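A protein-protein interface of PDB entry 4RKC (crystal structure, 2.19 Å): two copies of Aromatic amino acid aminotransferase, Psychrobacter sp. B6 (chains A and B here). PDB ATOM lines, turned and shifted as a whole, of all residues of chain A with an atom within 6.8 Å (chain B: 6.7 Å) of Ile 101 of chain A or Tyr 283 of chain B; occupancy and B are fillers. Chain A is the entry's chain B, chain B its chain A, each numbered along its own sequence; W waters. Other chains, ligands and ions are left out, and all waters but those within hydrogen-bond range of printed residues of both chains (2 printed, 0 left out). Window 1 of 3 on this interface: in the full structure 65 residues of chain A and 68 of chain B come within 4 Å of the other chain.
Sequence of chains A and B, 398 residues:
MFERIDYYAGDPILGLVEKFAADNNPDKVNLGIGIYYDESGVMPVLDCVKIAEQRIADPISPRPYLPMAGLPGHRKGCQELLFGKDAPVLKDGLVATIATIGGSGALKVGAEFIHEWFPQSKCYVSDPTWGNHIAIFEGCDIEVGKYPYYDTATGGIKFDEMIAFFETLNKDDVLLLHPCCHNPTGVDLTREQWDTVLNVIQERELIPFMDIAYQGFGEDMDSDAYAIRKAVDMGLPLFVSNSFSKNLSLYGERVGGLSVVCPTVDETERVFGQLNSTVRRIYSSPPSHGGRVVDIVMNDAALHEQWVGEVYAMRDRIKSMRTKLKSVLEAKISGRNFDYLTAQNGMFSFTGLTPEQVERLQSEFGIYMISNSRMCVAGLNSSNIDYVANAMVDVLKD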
ATOM      1  N   ALA A  99       0.646  21.259  18.528  1.00  0.00           N
ATOM      2  CA  ALA A  99       1.434  22.481  18.779  1.00  0.00           C
ATOM      3  C   ALA A  99       2.778  22.433  18.052  1.00  0.00           C
ATOM      4  O   ALA A  99       3.456  21.367  17.936  1.00  0.00           O
ATOM      5  CB  ALA A  99       1.620  22.763  20.248  1.00  0.00           C
ATOM      6  N   THR A 100       3.194  23.624  17.602  1.00  0.00           N
ATOM      7  CA  THR A 100       4.404  23.755  16.869  1.00  0.00           C
ATOM      8  C   THR A 100       5.269  24.926  17.334  1.00  0.00           C
ATOM      9  O   THR A 100       4.769  25.830  18.064  1.00  0.00           O
ATOM     10  CB  THR A 100       4.055  23.965  15.418  1.00  0.00           C
ATOM     11  OG1 THR A 100       3.246  25.147  15.317  1.00  0.00           O
ATOM     12  CG2 THR A 100       3.331  22.681  14.867  1.00  0.00           C
ATOM     13  N   ILE A 101       6.545  24.945  16.879  1.00  0.00           N
ATOM     14  CA  ILE A 101       7.495  26.016  17.254  1.00  0.00           C
ATOM     15  C   ILE A 101       7.178  27.167  16.276  1.00  0.00           C
ATOM     16  O   ILE A 101       7.857  27.361  15.260  1.00  0.00           O
ATOM     17  CB  ILE A 101       8.981  25.555  17.099  1.00  0.00           C
ATOM     18  CG1 ILE A 101       9.239  24.121  17.603  1.00  0.00           C
ATOM     19  CG2 ILE A 101       9.975  26.529  17.744  1.00  0.00           C
ATOM     20  CD1 ILE A 101       9.065  23.900  19.082  1.00  0.00           C
ATOM     21  N   GLY A 102       6.128  27.921  16.569  1.00  0.00           N
ATOM     22  CA  GLY A 102       5.640  28.941  15.686  1.00  0.00           C
ATOM     23  C   GLY A 102       5.012  28.333  14.458  1.00  0.00           C
ATOM     24  O   GLY A 102       4.872  27.093  14.286  1.00  0.00           O
ATOM     25  N   GLY A 103       4.626  29.215  13.561  1.00  0.00           N
ATOM     26  CA  GLY A 103       4.130  28.719  12.308  1.00  0.00           C
ATOM     27  C   GLY A 103       5.238  28.093  11.493  1.00  0.00           C
ATOM     28  O   GLY A 103       4.980  27.197  10.707  1.00  0.00           O
ATOM     29  N   SER A 104       6.448  28.614  11.613  1.00  0.00           N
ATOM     30  CA  SER A 104       7.634  28.043  10.951  1.00  0.00           C
ATOM     31  C   SER A 104       7.759  26.549  11.216  1.00  0.00           C
ATOM     32  O   SER A 104       7.909  25.792  10.308  1.00  0.00           O
ATOM     33  CB  SER A 104       8.905  28.733  11.492  1.00  0.00           C
ATOM     34  OG  SER A 104       8.851  30.051  11.056  1.00  0.00           O
ATOM     35  N   GLY A 105       7.732  26.180  12.495  1.00  0.00           N
ATOM     36  CA  GLY A 105       7.706  24.836  13.005  1.00  0.00           C
ATOM     37  C   GLY A 105       6.548  24.046  12.495  1.00  0.00           C
ATOM     38  O   GLY A 105       6.747  22.897  12.230  1.00  0.00           O
ATOM     39  N   ALA A 106       5.389  24.677  12.253  1.00  0.00           N
ATOM     40  CA  ALA A 106       4.218  23.990  11.701  1.00  0.00           C
ATOM     41  C   ALA A 106       4.447  23.683  10.240  1.00  0.00           C
ATOM     42  O   ALA A 106       4.110  22.567   9.766  1.00  0.00           O
ATOM     43  CB  ALA A 106       2.964  24.825  11.854  1.00  0.00           C
ATOM     44  N   LYS A 108       7.291  23.456   8.796  1.00  0.00           N
ATOM     45  CA  LYS A 108       8.368  22.444   8.764  1.00  0.00           C
ATOM     46  C   LYS A 108       7.830  20.967   8.973  1.00  0.00           C
ATOM     47  O   LYS A 108       8.193  20.035   8.201  1.00  0.00           O
ATOM     48  CB  LYS A 108       9.410  22.781   9.834  1.00  0.00           C
ATOM     49  CG  LYS A 108      10.503  21.712  10.042  1.00  0.00           C
ATOM     50  CD  LYS A 108      11.258  21.412   8.711  1.00  0.00           C
ATOM     51  CE  LYS A 108      12.583  20.678   8.880  1.00  0.00           C
ATOM     52  NZ  LYS A 108      13.160  20.394   7.540  1.00  0.00           N
ATOM     53  N   VAL A 109       7.047  20.739  10.029  1.00  0.00           N
ATOM     54  CA  VAL A 109       6.576  19.410  10.356  1.00  0.00           C
ATOM     55  C   VAL A 109       5.662  19.000   9.220  1.00  0.00           C
ATOM     56  O   VAL A 109       5.798  17.932   8.696  1.00  0.00           O
ATOM     57  CB  VAL A 109       5.817  19.424  11.711  1.00  0.00           C
ATOM     58  CG1 VAL A 109       5.024  18.092  11.929  1.00  0.00           C
ATOM     59  CG2 VAL A 109       6.823  19.640  12.847  1.00  0.00           C
ATOM     60  N   ASN A 132      11.127  32.896   3.880  1.00  0.00           N
ATOM     61  CA  ASN A 132      11.206  31.684   4.784  1.00  0.00           C
ATOM     62  C   ASN A 132      10.373  30.409   4.384  1.00  0.00           C
ATOM     63  O   ASN A 132      10.771  29.266   4.649  1.00  0.00           O
ATOM     64  CB  ASN A 132      10.947  32.014   6.263  1.00  0.00           C
ATOM     65  CG  ASN A 132      11.739  31.094   7.165  1.00  0.00           C
ATOM     66  OD1 ASN A 132      12.858  30.765   6.760  1.00  0.00           O
ATOM     67  ND2 ASN A 132      11.208  30.624   8.313  1.00  0.00           N
ATOM     68  N   ILE A 136      12.037  26.672   4.138  1.00  0.00           N
ATOM     69  CA  ILE A 136      11.505  25.529   4.921  1.00  0.00           C
ATOM     70  C   ILE A 136      11.137  24.270   4.042  1.00  0.00           C
ATOM     71  O   ILE A 136      11.508  23.108   4.354  1.00  0.00           O
ATOM     72  CB  ILE A 136      10.309  25.916   5.777  1.00  0.00           C
ATOM     73  CG1 ILE A 136      10.664  27.037   6.805  1.00  0.00           C
ATOM     74  CG2 ILE A 136       9.623  24.647   6.335  1.00  0.00           C
ATOM     75  CD1 ILE A 136       9.362  27.618   7.399  1.00  0.00           C
ATOM     76  N   GLU A 253       8.301  33.212  21.990  1.00  0.00           N
ATOM     77  CA  GLU A 253       7.980  31.975  22.717  1.00  0.00           C
ATOM     78  C   GLU A 253       7.700  30.787  21.773  1.00  0.00           C
ATOM     79  O   GLU A 253       7.594  29.673  22.266  1.00  0.00           O
ATOM     80  CB  GLU A 253       6.774  32.102  23.633  1.00  0.00           C
ATOM     81  CG  GLU A 253       6.940  33.180  24.687  1.00  0.00           C
ATOM     82  CD  GLU A 253       8.054  32.881  25.683  1.00  0.00           C
ATOM     83  OE1 GLU A 253       8.354  33.767  26.443  1.00  0.00           O
ATOM     84  OE2 GLU A 253       8.627  31.770  25.712  1.00  0.00           O
ATOM     85  N   ARG A 254       7.551  31.049  20.444  1.00  0.00           N
ATOM     86  CA  ARG A 254       7.394  30.042  19.395  1.00  0.00           C
ATOM     87  C   ARG A 254       6.131  29.234  19.555  1.00  0.00           C
ATOM     88  O   ARG A 254       6.167  28.023  19.934  1.00  0.00           O
ATOM     89  CB  ARG A 254       8.640  29.122  19.236  1.00  0.00           C
ATOM     90  CG  ARG A 254       9.936  29.884  19.437  1.00  0.00           C
ATOM     91  CD  ARG A 254      10.092  31.127  18.582  1.00  0.00           C
ATOM     92  NE  ARG A 254      10.091  30.652  17.211  1.00  0.00           N
ATOM     93  CZ  ARG A 254       9.177  30.973  16.291  1.00  0.00           C
ATOM     94  NH1 ARG A 254       8.129  31.769  16.570  1.00  0.00           N
ATOM     95  NH2 ARG A 254       9.278  30.399  15.104  1.00  0.00           N
ATOM     96  N   VAL A 255       5.000  29.863  19.226  1.00  0.00           N
ATOM     97  CA  VAL A 255       3.781  29.179  19.454  1.00  0.00           C
ATOM     98  C   VAL A 255       2.956  29.194  18.170  1.00  0.00           C
ATOM     99  O   VAL A 255       2.640  30.239  17.643  1.00  0.00           O
ATOM    100  CB  VAL A 255       3.027  29.844  20.586  1.00  0.00           C
ATOM    101  CG1 VAL A 255       3.602  29.389  21.908  1.00  0.00           C
ATOM    102  CG2 VAL A 255       3.077  31.388  20.438  1.00  0.00           C
ATOM    103  N   GLY A 256       2.669  27.992  17.659  1.00  0.00           N
ATOM    104  CA  GLY A 256       1.782  27.878  16.547  1.00  0.00           C
ATOM    105  C   GLY A 256       1.100  26.543  16.581  1.00  0.00           C
ATOM    106  O   GLY A 256       1.169  25.830  17.601  1.00  0.00           O
ATOM    107  N   GLY A 257       0.421  26.222  15.470  1.00  0.00           N
ATOM    108  CA  GLY A 257      -0.133  24.910  15.324  1.00  0.00           C
ATOM    109  C   GLY A 257      -0.020  24.411  13.913  1.00  0.00           C
ATOM    110  O   GLY A 257       0.142  25.186  12.944  1.00  0.00           O
ATOM    111  N   ILE A 282      12.574  15.574  15.295  1.00  0.00           N
ATOM    112  CA  ILE A 282      13.033  16.944  15.166  1.00  0.00           C
ATOM    113  C   ILE A 282      13.400  17.680  16.492  1.00  0.00           C
ATOM    114  O   ILE A 282      14.547  18.223  16.655  1.00  0.00           O
ATOM    115  CB  ILE A 282      12.065  17.801  14.349  1.00  0.00           C
ATOM    116  CG1 ILE A 282      11.752  17.197  12.933  1.00  0.00           C
ATOM    117  CG2 ILE A 282      12.666  19.221  14.137  1.00  0.00           C
ATOM    118  CD1 ILE A 282      10.719  18.045  12.221  1.00  0.00           C
ATOM    119  N   TYR A 283      12.483  17.802  17.449  1.00  0.00           N
ATOM    120  CA  TYR A 283      12.839  18.561  18.708  1.00  0.00           C
ATOM    121  C   TYR A 283      12.231  17.903  19.936  1.00  0.00           C
ATOM    122  O   TYR A 283      12.243  18.502  21.041  1.00  0.00           O
ATOM    123  CB  TYR A 283      12.367  20.013  18.657  1.00  0.00           C
ATOM    124  CG  TYR A 283      10.966  20.188  18.236  1.00  0.00           C
ATOM    125  CD1 TYR A 283      10.644  20.306  16.859  1.00  0.00           C
ATOM    126  CD2 TYR A 283       9.941  20.277  19.159  1.00  0.00           C
ATOM    127  CE1 TYR A 283       9.333  20.415  16.457  1.00  0.00           C
ATOM    128  CE2 TYR A 283       8.614  20.401  18.751  1.00  0.00           C
ATOM    129  CZ  TYR A 283       8.332  20.479  17.395  1.00  0.00           C
ATOM    130  OH  TYR A 283       7.023  20.591  16.911  1.00  0.00           O
ATOM    131  N   SER A 285       9.619  17.615  21.697  1.00  0.00           N
ATOM    132  CA  SER A 285       8.380  18.181  22.158  1.00  0.00           C
ATOM    133  C   SER A 285       8.528  19.701  22.319  1.00  0.00           C
ATOM    134  O   SER A 285       9.661  20.238  22.349  1.00  0.00           O
ATOM    135  CB  SER A 285       8.001  17.543  23.524  1.00  0.00           C
ATOM    136  OG  SER A 285       8.924  17.959  24.518  1.00  0.00           O
ATOM    137  N   PRO A 286       7.400  20.419  22.312  1.00  0.00           N
ATOM    138  CA  PRO A 286       7.427  21.831  22.175  1.00  0.00           C
ATOM    139  C   PRO A 286       7.493  22.559  23.502  1.00  0.00           C
ATOM    140  O   PRO A 286       7.342  21.950  24.571  1.00  0.00           O
ATOM    141  CB  PRO A 286       6.050  22.123  21.529  1.00  0.00           C
ATOM    142  CG  PRO A 286       5.180  21.140  22.222  1.00  0.00           C
ATOM    143  CD  PRO A 286       6.011  19.895  22.209  1.00  0.00           C
ATOM    144  N   PRO A 287       7.698  23.916  23.445  1.00  0.00           N
ATOM    145  CA  PRO A 287       7.983  24.623  24.680  1.00  0.00           C
ATOM    146  C   PRO A 287       6.800  24.870  25.562  1.00  0.00           C
ATOM    147  O   PRO A 287       5.665  25.270  25.107  1.00  0.00           O
ATOM    148  CB  PRO A 287       8.666  25.940  24.209  1.00  0.00           C
ATOM    149  CG  PRO A 287       8.409  26.026  22.779  1.00  0.00           C
ATOM    150  CD  PRO A 287       8.066  24.683  22.243  1.00  0.00           C
ATOM    151  N   MET B  68      18.340  33.786  15.708  1.00  0.00           N
ATOM    152  CA  MET B  68      18.347  32.361  15.310  1.00  0.00           C
ATOM    153  C   MET B  68      19.200  31.478  16.243  1.00  0.00           C
ATOM    154  O   MET B  68      18.783  30.376  16.592  1.00  0.00           O
ATOM    155  CB  MET B  68      18.770  32.215  13.858  1.00  0.00           C
ATOM    156  CG  MET B  68      17.678  32.487  12.800  1.00  0.00           C
ATOM    157  SD  MET B  68      18.429  32.599  11.162  1.00  0.00           S
ATOM    158  CE  MET B  68      19.551  34.005  11.215  1.00  0.00           C
ATOM    159  N   ILE B  98      24.970  27.441  19.016  1.00  0.00           N
ATOM    160  CA  ILE B  98      23.618  27.981  19.058  1.00  0.00           C
ATOM    161  C   ILE B  98      22.840  27.424  20.272  1.00  0.00           C
ATOM    162  O   ILE B  98      23.097  26.277  20.697  1.00  0.00           O
ATOM    163  CB  ILE B  98      22.848  27.617  17.779  1.00  0.00           C
ATOM    164  CG1 ILE B  98      22.793  26.080  17.561  1.00  0.00           C
ATOM    165  CG2 ILE B  98      23.490  28.279  16.570  1.00  0.00           C
ATOM    166  CD1 ILE B  98      21.790  25.690  16.446  1.00  0.00           C
ATOM    167  N   ALA B  99      21.855  28.188  20.772  1.00  0.00           N
ATOM    168  CA  ALA B  99      20.836  27.600  21.636  1.00  0.00           C
ATOM    169  C   ALA B  99      19.991  26.668  20.802  1.00  0.00           C
ATOM    170  O   ALA B  99      19.805  26.884  19.594  1.00  0.00           O
ATOM    171  CB  ALA B  99      19.962  28.668  22.274  1.00  0.00           C
ATOM    172  N   THR B 100      19.465  25.605  21.419  1.00  0.00           N
ATOM    173  CA  THR B 100      18.698  24.653  20.574  1.00  0.00           C
ATOM    174  C   THR B 100      17.466  24.255  21.351  1.00  0.00           C
ATOM    175  O   THR B 100      17.409  24.521  22.559  1.00  0.00           O
ATOM    176  CB  THR B 100      19.565  23.412  20.309  1.00  0.00           C
ATOM    177  OG1 THR B 100      19.964  22.861  21.570  1.00  0.00           O
ATOM    178  CG2 THR B 100      20.777  23.753  19.587  1.00  0.00           C
ATOM    179  N   ILE B 101      16.518  23.571  20.680  1.00  0.00           N
ATOM    180  CA  ILE B 101      15.256  23.130  21.322  1.00  0.00           C
ATOM    181  C   ILE B 101      15.555  21.828  22.063  1.00  0.00           C
ATOM    182  O   ILE B 101      15.434  20.747  21.480  1.00  0.00           O
ATOM    183  CB  ILE B 101      14.113  22.851  20.332  1.00  0.00           C
ATOM    184  CG1 ILE B 101      13.974  23.955  19.301  1.00  0.00           C
ATOM    185  CG2 ILE B 101      12.784  22.536  21.051  1.00  0.00           C
ATOM    186  CD1 ILE B 101      14.071  25.304  19.933  1.00  0.00           C
ATOM    187  N   GLY B 105      16.848  19.070  19.830  1.00  0.00           N
ATOM    188  CA  GLY B 105      17.075  19.941  18.697  1.00  0.00           C
ATOM    189  C   GLY B 105      18.520  20.160  18.300  1.00  0.00           C
ATOM    190  O   GLY B 105      18.754  20.491  17.125  1.00  0.00           O
ATOM    191  N   ALA B 106      19.485  20.103  19.248  1.00  0.00           N
ATOM    192  CA  ALA B 106      20.946  20.140  18.985  1.00  0.00           C
ATOM    193  C   ALA B 106      21.402  18.960  18.113  1.00  0.00           C
ATOM    194  O   ALA B 106      22.023  19.157  17.075  1.00  0.00           O
ATOM    195  CB  ALA B 106      21.759  20.194  20.314  1.00  0.00           C
ATOM    196  N   VAL B 109      19.886  19.655  14.704  1.00  0.00           N
ATOM    197  CA  VAL B 109      20.501  20.663  13.851  1.00  0.00           C
ATOM    198  C   VAL B 109      21.873  20.143  13.450  1.00  0.00           C
ATOM    199  O   VAL B 109      22.295  20.282  12.297  1.00  0.00           O
ATOM    200  CB  VAL B 109      20.663  22.044  14.548  1.00  0.00           C
ATOM    201  CG1 VAL B 109      21.722  22.931  13.798  1.00  0.00           C
ATOM    202  CG2 VAL B 109      19.307  22.752  14.605  1.00  0.00           C
ATOM    203  N   ARG B 254      12.554  23.177  26.824  1.00  0.00           N
ATOM    204  CA  ARG B 254      13.363  22.893  25.597  1.00  0.00           C
ATOM    205  C   ARG B 254      14.633  23.757  25.501  1.00  0.00           C
ATOM    206  O   ARG B 254      14.716  24.624  24.607  1.00  0.00           O
ATOM    207  CB  ARG B 254      12.477  23.031  24.307  1.00  0.00           C
ATOM    208  CG  ARG B 254      11.028  22.520  24.473  1.00  0.00           C
ATOM    209  CD  ARG B 254      11.014  21.111  25.044  1.00  0.00           C
ATOM    210  NE  ARG B 254      11.713  20.177  24.153  1.00  0.00           N
ATOM    211  CZ  ARG B 254      12.816  19.515  24.463  1.00  0.00           C
ATOM    212  NH1 ARG B 254      13.366  19.643  25.675  1.00  0.00           N
ATOM    213  NH2 ARG B 254      13.398  18.768  23.554  1.00  0.00           N
ATOM    214  N   THR B 278      20.445  26.609   9.159  1.00  0.00           N
ATOM    215  CA  THR B 278      19.749  25.339   9.432  1.00  0.00           C
ATOM    216  C   THR B 278      18.661  25.585  10.470  1.00  0.00           C
ATOM    217  O   THR B 278      17.508  25.182  10.289  1.00  0.00           O
ATOM    218  CB  THR B 278      20.746  24.284   9.935  1.00  0.00           C
ATOM    219  OG1 THR B 278      21.699  24.058   8.889  1.00  0.00           O
ATOM    220  CG2 THR B 278      20.039  22.965  10.291  1.00  0.00           C
ATOM    221  N   VAL B 279      18.971  26.310  11.552  1.00  0.00           N
ATOM    222  CA  VAL B 279      17.861  26.756  12.433  1.00  0.00           C
ATOM    223  C   VAL B 279      16.713  27.426  11.633  1.00  0.00           C
ATOM    224  O   VAL B 279      15.522  27.089  11.817  1.00  0.00           O
ATOM    225  CB  VAL B 279      18.317  27.711  13.518  1.00  0.00           C
ATOM    226  CG1 VAL B 279      17.129  28.424  14.183  1.00  0.00           C
ATOM    227  CG2 VAL B 279      19.109  26.892  14.524  1.00  0.00           C
ATOM    228  N   ARG B 280      17.045  28.380  10.764  1.00  0.00           N
ATOM    229  CA  ARG B 280      16.037  29.176  10.091  1.00  0.00           C
ATOM    230  C   ARG B 280      15.041  28.335   9.356  1.00  0.00           C
ATOM    231  O   ARG B 280      13.783  28.655   9.353  1.00  0.00           O
ATOM    232  CB  ARG B 280      16.696  30.121   9.088  1.00  0.00           C
ATOM    233  CG  ARG B 280      15.756  31.176   8.495  1.00  0.00           C
ATOM    234  CD  ARG B 280      16.526  32.213   7.672  1.00  0.00           C
ATOM    235  NE  ARG B 280      15.629  33.163   6.995  1.00  0.00           N
ATOM    236  CZ  ARG B 280      15.055  32.974   5.794  1.00  0.00           C
ATOM    237  NH1 ARG B 280      15.234  31.858   5.069  1.00  0.00           N
ATOM    238  NH2 ARG B 280      14.300  33.929   5.319  1.00  0.00           N
ATOM    239  N   ARG B 281      15.530  27.255   8.726  1.00  0.00           N
ATOM    240  CA  ARG B 281      14.655  26.514   7.812  1.00  0.00           C
ATOM    241  C   ARG B 281      13.864  25.456   8.588  1.00  0.00           C
ATOM    242  O   ARG B 281      13.151  24.704   7.996  1.00  0.00           O
ATOM    243  CB  ARG B 281      15.474  25.841   6.667  1.00  0.00           C
ATOM    244  CG  ARG B 281      16.287  24.636   7.176  1.00  0.00           C
ATOM    245  CD  ARG B 281      17.342  24.180   6.172  1.00  0.00           C
ATOM    246  NE  ARG B 281      18.363  25.190   5.962  1.00  0.00           N
ATOM    247  CZ  ARG B 281      19.524  24.958   5.337  1.00  0.00           C
ATOM    248  NH1 ARG B 281      19.741  23.763   4.847  1.00  0.00           N
ATOM    249  NH2 ARG B 281      20.455  25.923   5.191  1.00  0.00           N
ATOM    250  N   ILE B 282      14.103  25.365   9.894  1.00  0.00           N
ATOM    251  CA  ILE B 282      13.459  24.405  10.734  1.00  0.00           C
ATOM    252  C   ILE B 282      12.399  25.084  11.618  1.00  0.00           C
ATOM    253  O   ILE B 282      11.178  24.715  11.543  1.00  0.00           O
ATOM    254  CB  ILE B 282      14.413  23.461  11.568  1.00  0.00           C
ATOM    255  CG1 ILE B 282      15.458  22.671  10.708  1.00  0.00           C
ATOM    256  CG2 ILE B 282      13.629  22.412  12.434  1.00  0.00           C
ATOM    257  CD1 ILE B 282      16.424  21.899  11.539  1.00  0.00           C
ATOM    258  N   TYR B 283      12.805  26.002  12.500  1.00  0.00           N
ATOM    259  CA  TYR B 283      11.814  26.548  13.415  1.00  0.00           C
ATOM    260  C   TYR B 283      11.996  28.047  13.610  1.00  0.00           C
ATOM    261  O   TYR B 283      11.369  28.646  14.512  1.00  0.00           O
ATOM    262  CB  TYR B 283      11.924  25.864  14.761  1.00  0.00           C
ATOM    263  CG  TYR B 283      13.324  25.847  15.349  1.00  0.00           C
ATOM    264  CD1 TYR B 283      14.154  24.734  15.179  1.00  0.00           C
ATOM    265  CD2 TYR B 283      13.783  26.905  16.116  1.00  0.00           C
ATOM    266  CE1 TYR B 283      15.400  24.680  15.725  1.00  0.00           C
ATOM    267  CE2 TYR B 283      15.029  26.860  16.678  1.00  0.00           C
ATOM    268  CZ  TYR B 283      15.844  25.786  16.433  1.00  0.00           C
ATOM    269  OH  TYR B 283      17.069  25.678  16.967  1.00  0.00           O
ATOM    270  N   SER B 284      12.872  28.591  12.781  1.00  0.00           N
ATOM    271  CA  SER B 284      13.205  29.989  12.684  1.00  0.00           C
ATOM    272  C   SER B 284      14.086  30.559  13.874  1.00  0.00           C
ATOM    273  O   SER B 284      15.100  31.163  13.669  1.00  0.00           O
ATOM    274  CB  SER B 284      11.928  30.730  12.408  1.00  0.00           C
ATOM    275  OG  SER B 284      12.241  32.048  12.287  1.00  0.00           O
ATOM    276  N   SER B 285      13.683  30.383  15.115  1.00  0.00           N
ATOM    277  CA  SER B 285      14.503  30.747  16.274  1.00  0.00           C
ATOM    278  C   SER B 285      13.899  30.055  17.483  1.00  0.00           C
ATOM    279  O   SER B 285      12.706  29.639  17.480  1.00  0.00           O
ATOM    280  CB  SER B 285      14.445  32.263  16.499  1.00  0.00           C
ATOM    281  OG  SER B 285      13.121  32.714  16.665  1.00  0.00           O
ATOM    282  N   PRO B 286      14.691  29.988  18.554  1.00  0.00           N
ATOM    283  CA  PRO B 286      14.303  29.168  19.691  1.00  0.00           C
ATOM    284  C   PRO B 286      13.513  29.942  20.744  1.00  0.00           C
ATOM    285  O   PRO B 286      13.460  31.167  20.689  1.00  0.00           O
ATOM    286  CB  PRO B 286      15.686  28.747  20.270  1.00  0.00           C
ATOM    287  CG  PRO B 286      16.494  29.974  20.054  1.00  0.00           C
ATOM    288  CD  PRO B 286      16.156  30.347  18.622  1.00  0.00           C
ATOM    289  N   PRO B 287      12.933  29.231  21.747  1.00  0.00           N
ATOM    290  CA  PRO B 287      12.031  29.868  22.735  1.00  0.00           C
ATOM    291  C   PRO B 287      12.700  30.771  23.723  1.00  0.00           C
ATOM    292  O   PRO B 287      13.663  30.409  24.357  1.00  0.00           O
ATOM    293  CB  PRO B 287      11.321  28.724  23.441  1.00  0.00           C
ATOM    294  CG  PRO B 287      11.991  27.477  22.975  1.00  0.00           C
ATOM    295  CD  PRO B 287      12.990  27.781  21.862  1.00  0.00           C
HETATM  296  O   HOH W   1      12.653  33.109   9.643  1.00  0.00           O
HETATM  297  O   HOH W   2      13.409  22.791   6.160  1.00  0.00           O
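The backbone carbonyl oxygen of Tyr 283 of chain A lies within hydrogen-bond range of the guanidinium group of Arg 254 of chain B, 2.8 Å away. The guanidinium group (NE) of Arg 254 of chain B is in hydrogen-bond range of the backbone carbonyl oxygen (O) of Ser 285 of chain A, at 2.7 Å. OD1 of Asn 132 of chain A lies within hydrogen-bond range of NH1 of Arg 280 of chain B (3.1 Å). The guanidinium group (NH2) of Arg 254 of chain A lies within hydrogen-bond range of the backbone carbonyl oxygen (O) of Tyr 283 of chain B, at 2.8 Å. The backbone carbonyl oxygen (O) of Ser 285 of chain B is in hydrogen-bond range of the guanidinium group (NE) of Arg 254 of chain A, 2.8 Å away.
O of Val 279 of chain B sits at hydrogen-bond distance from N of Ser 284 of chain B, at 3.2 Å. O of Ile 101 of chain A is in hydrogen-bond range of NH2 of Arg 254 of chain A. The backbone NH (N) of Gly 102 of chain A sits close to the backbone carbonyl oxygen (O) of Arg 254 of chain A, at 3.4 Å.
Among the printed residues, pairs that only touch across the chains: Ile 101 of chain A with Tyr 283 of chain B (3.6 Å), Ser 104 of chain A with Ile 282 of chain B (3.7 Å), Ser 104 of chain A with Tyr 283 of chain B (3.8 Å), Ser 104 of chain A with Ser 284 of chain B (3.4 Å), Gly 105 of chain A with Ile 282 of chain B (3.8 Å), Lys 108 of chain A with Arg 281 of chain B (3.9 Å), Lys 108 of chain A with Ile 282 of chain B (3.1 Å), Ile 136 of chain A with Arg 281 of chain B (3.6 Å), Arg 254 of chain A with Ser 284 of chain B (3.8 Å), Arg 254 of chain A with Pro 286 of chain B (3.8 Å), Arg 254 of chain A with Pro 287 of chain B (3.8 Å), Ile 282 of chain A with Gly 105 of chain B (3.7 Å), Ile 282 of chain A with Ile 282 of chain B (3.7 Å), Tyr 283 of chain A with Ile 101 of chain B (3.5 Å), Pro 286 of chain A with Arg 254 of chain B (3.7 Å), Pro 287 of chain A with Arg 254 of chain B (3.7 Å) and Pro 287 of chain A with Pro 287 of chain B (3.9 Å).
Ile 101 of chain A touches one residue of chain B. Printed residues of chain B within 4 Å of Lys 108 of chain A: Arg 281 (3.9 Å) and Ile 282 (3.1 Å). Of the printed residues of chain B, Asn 132 of chain A touches Arg 280 (3.1 Å). Printed residues of chain B within 4 Å of Ile 136 of chain A: Arg 281. The nearest residue of chain B that does not touch Ile 101 of chain A is Ser 285 of chain B (4.1 Å). The nearest residue of chain A that does not touch Tyr 283 of chain B is Gly 105 of chain A (4.2 Å). The nearest printed residue of chain B that does not touch Ile 136 of chain A is Arg 280 of chain B (4.3 Å).
Hydrophobic or aromatic side chains of chain B within 4 Å of the printed part of chain A: Ile 101, Ile 282, Tyr 283 and Pro 287. Of the 22 printed residues of chain A, 12 touch a printed residue of chain B. Among the printed residues, 22 pairs touch across the chains.
Ile 282 of chain A touches its own counterpart, Ile 282 of chain B. Positions printed for both chains: 99, 100, 101, 105, 106, 109, 254, 282, 283, 285, 286 and 287.
Water W1 lies within hydrogen-bond range of OG of Ser 284 of chain B and ND2 of Asn 132 of chain A.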
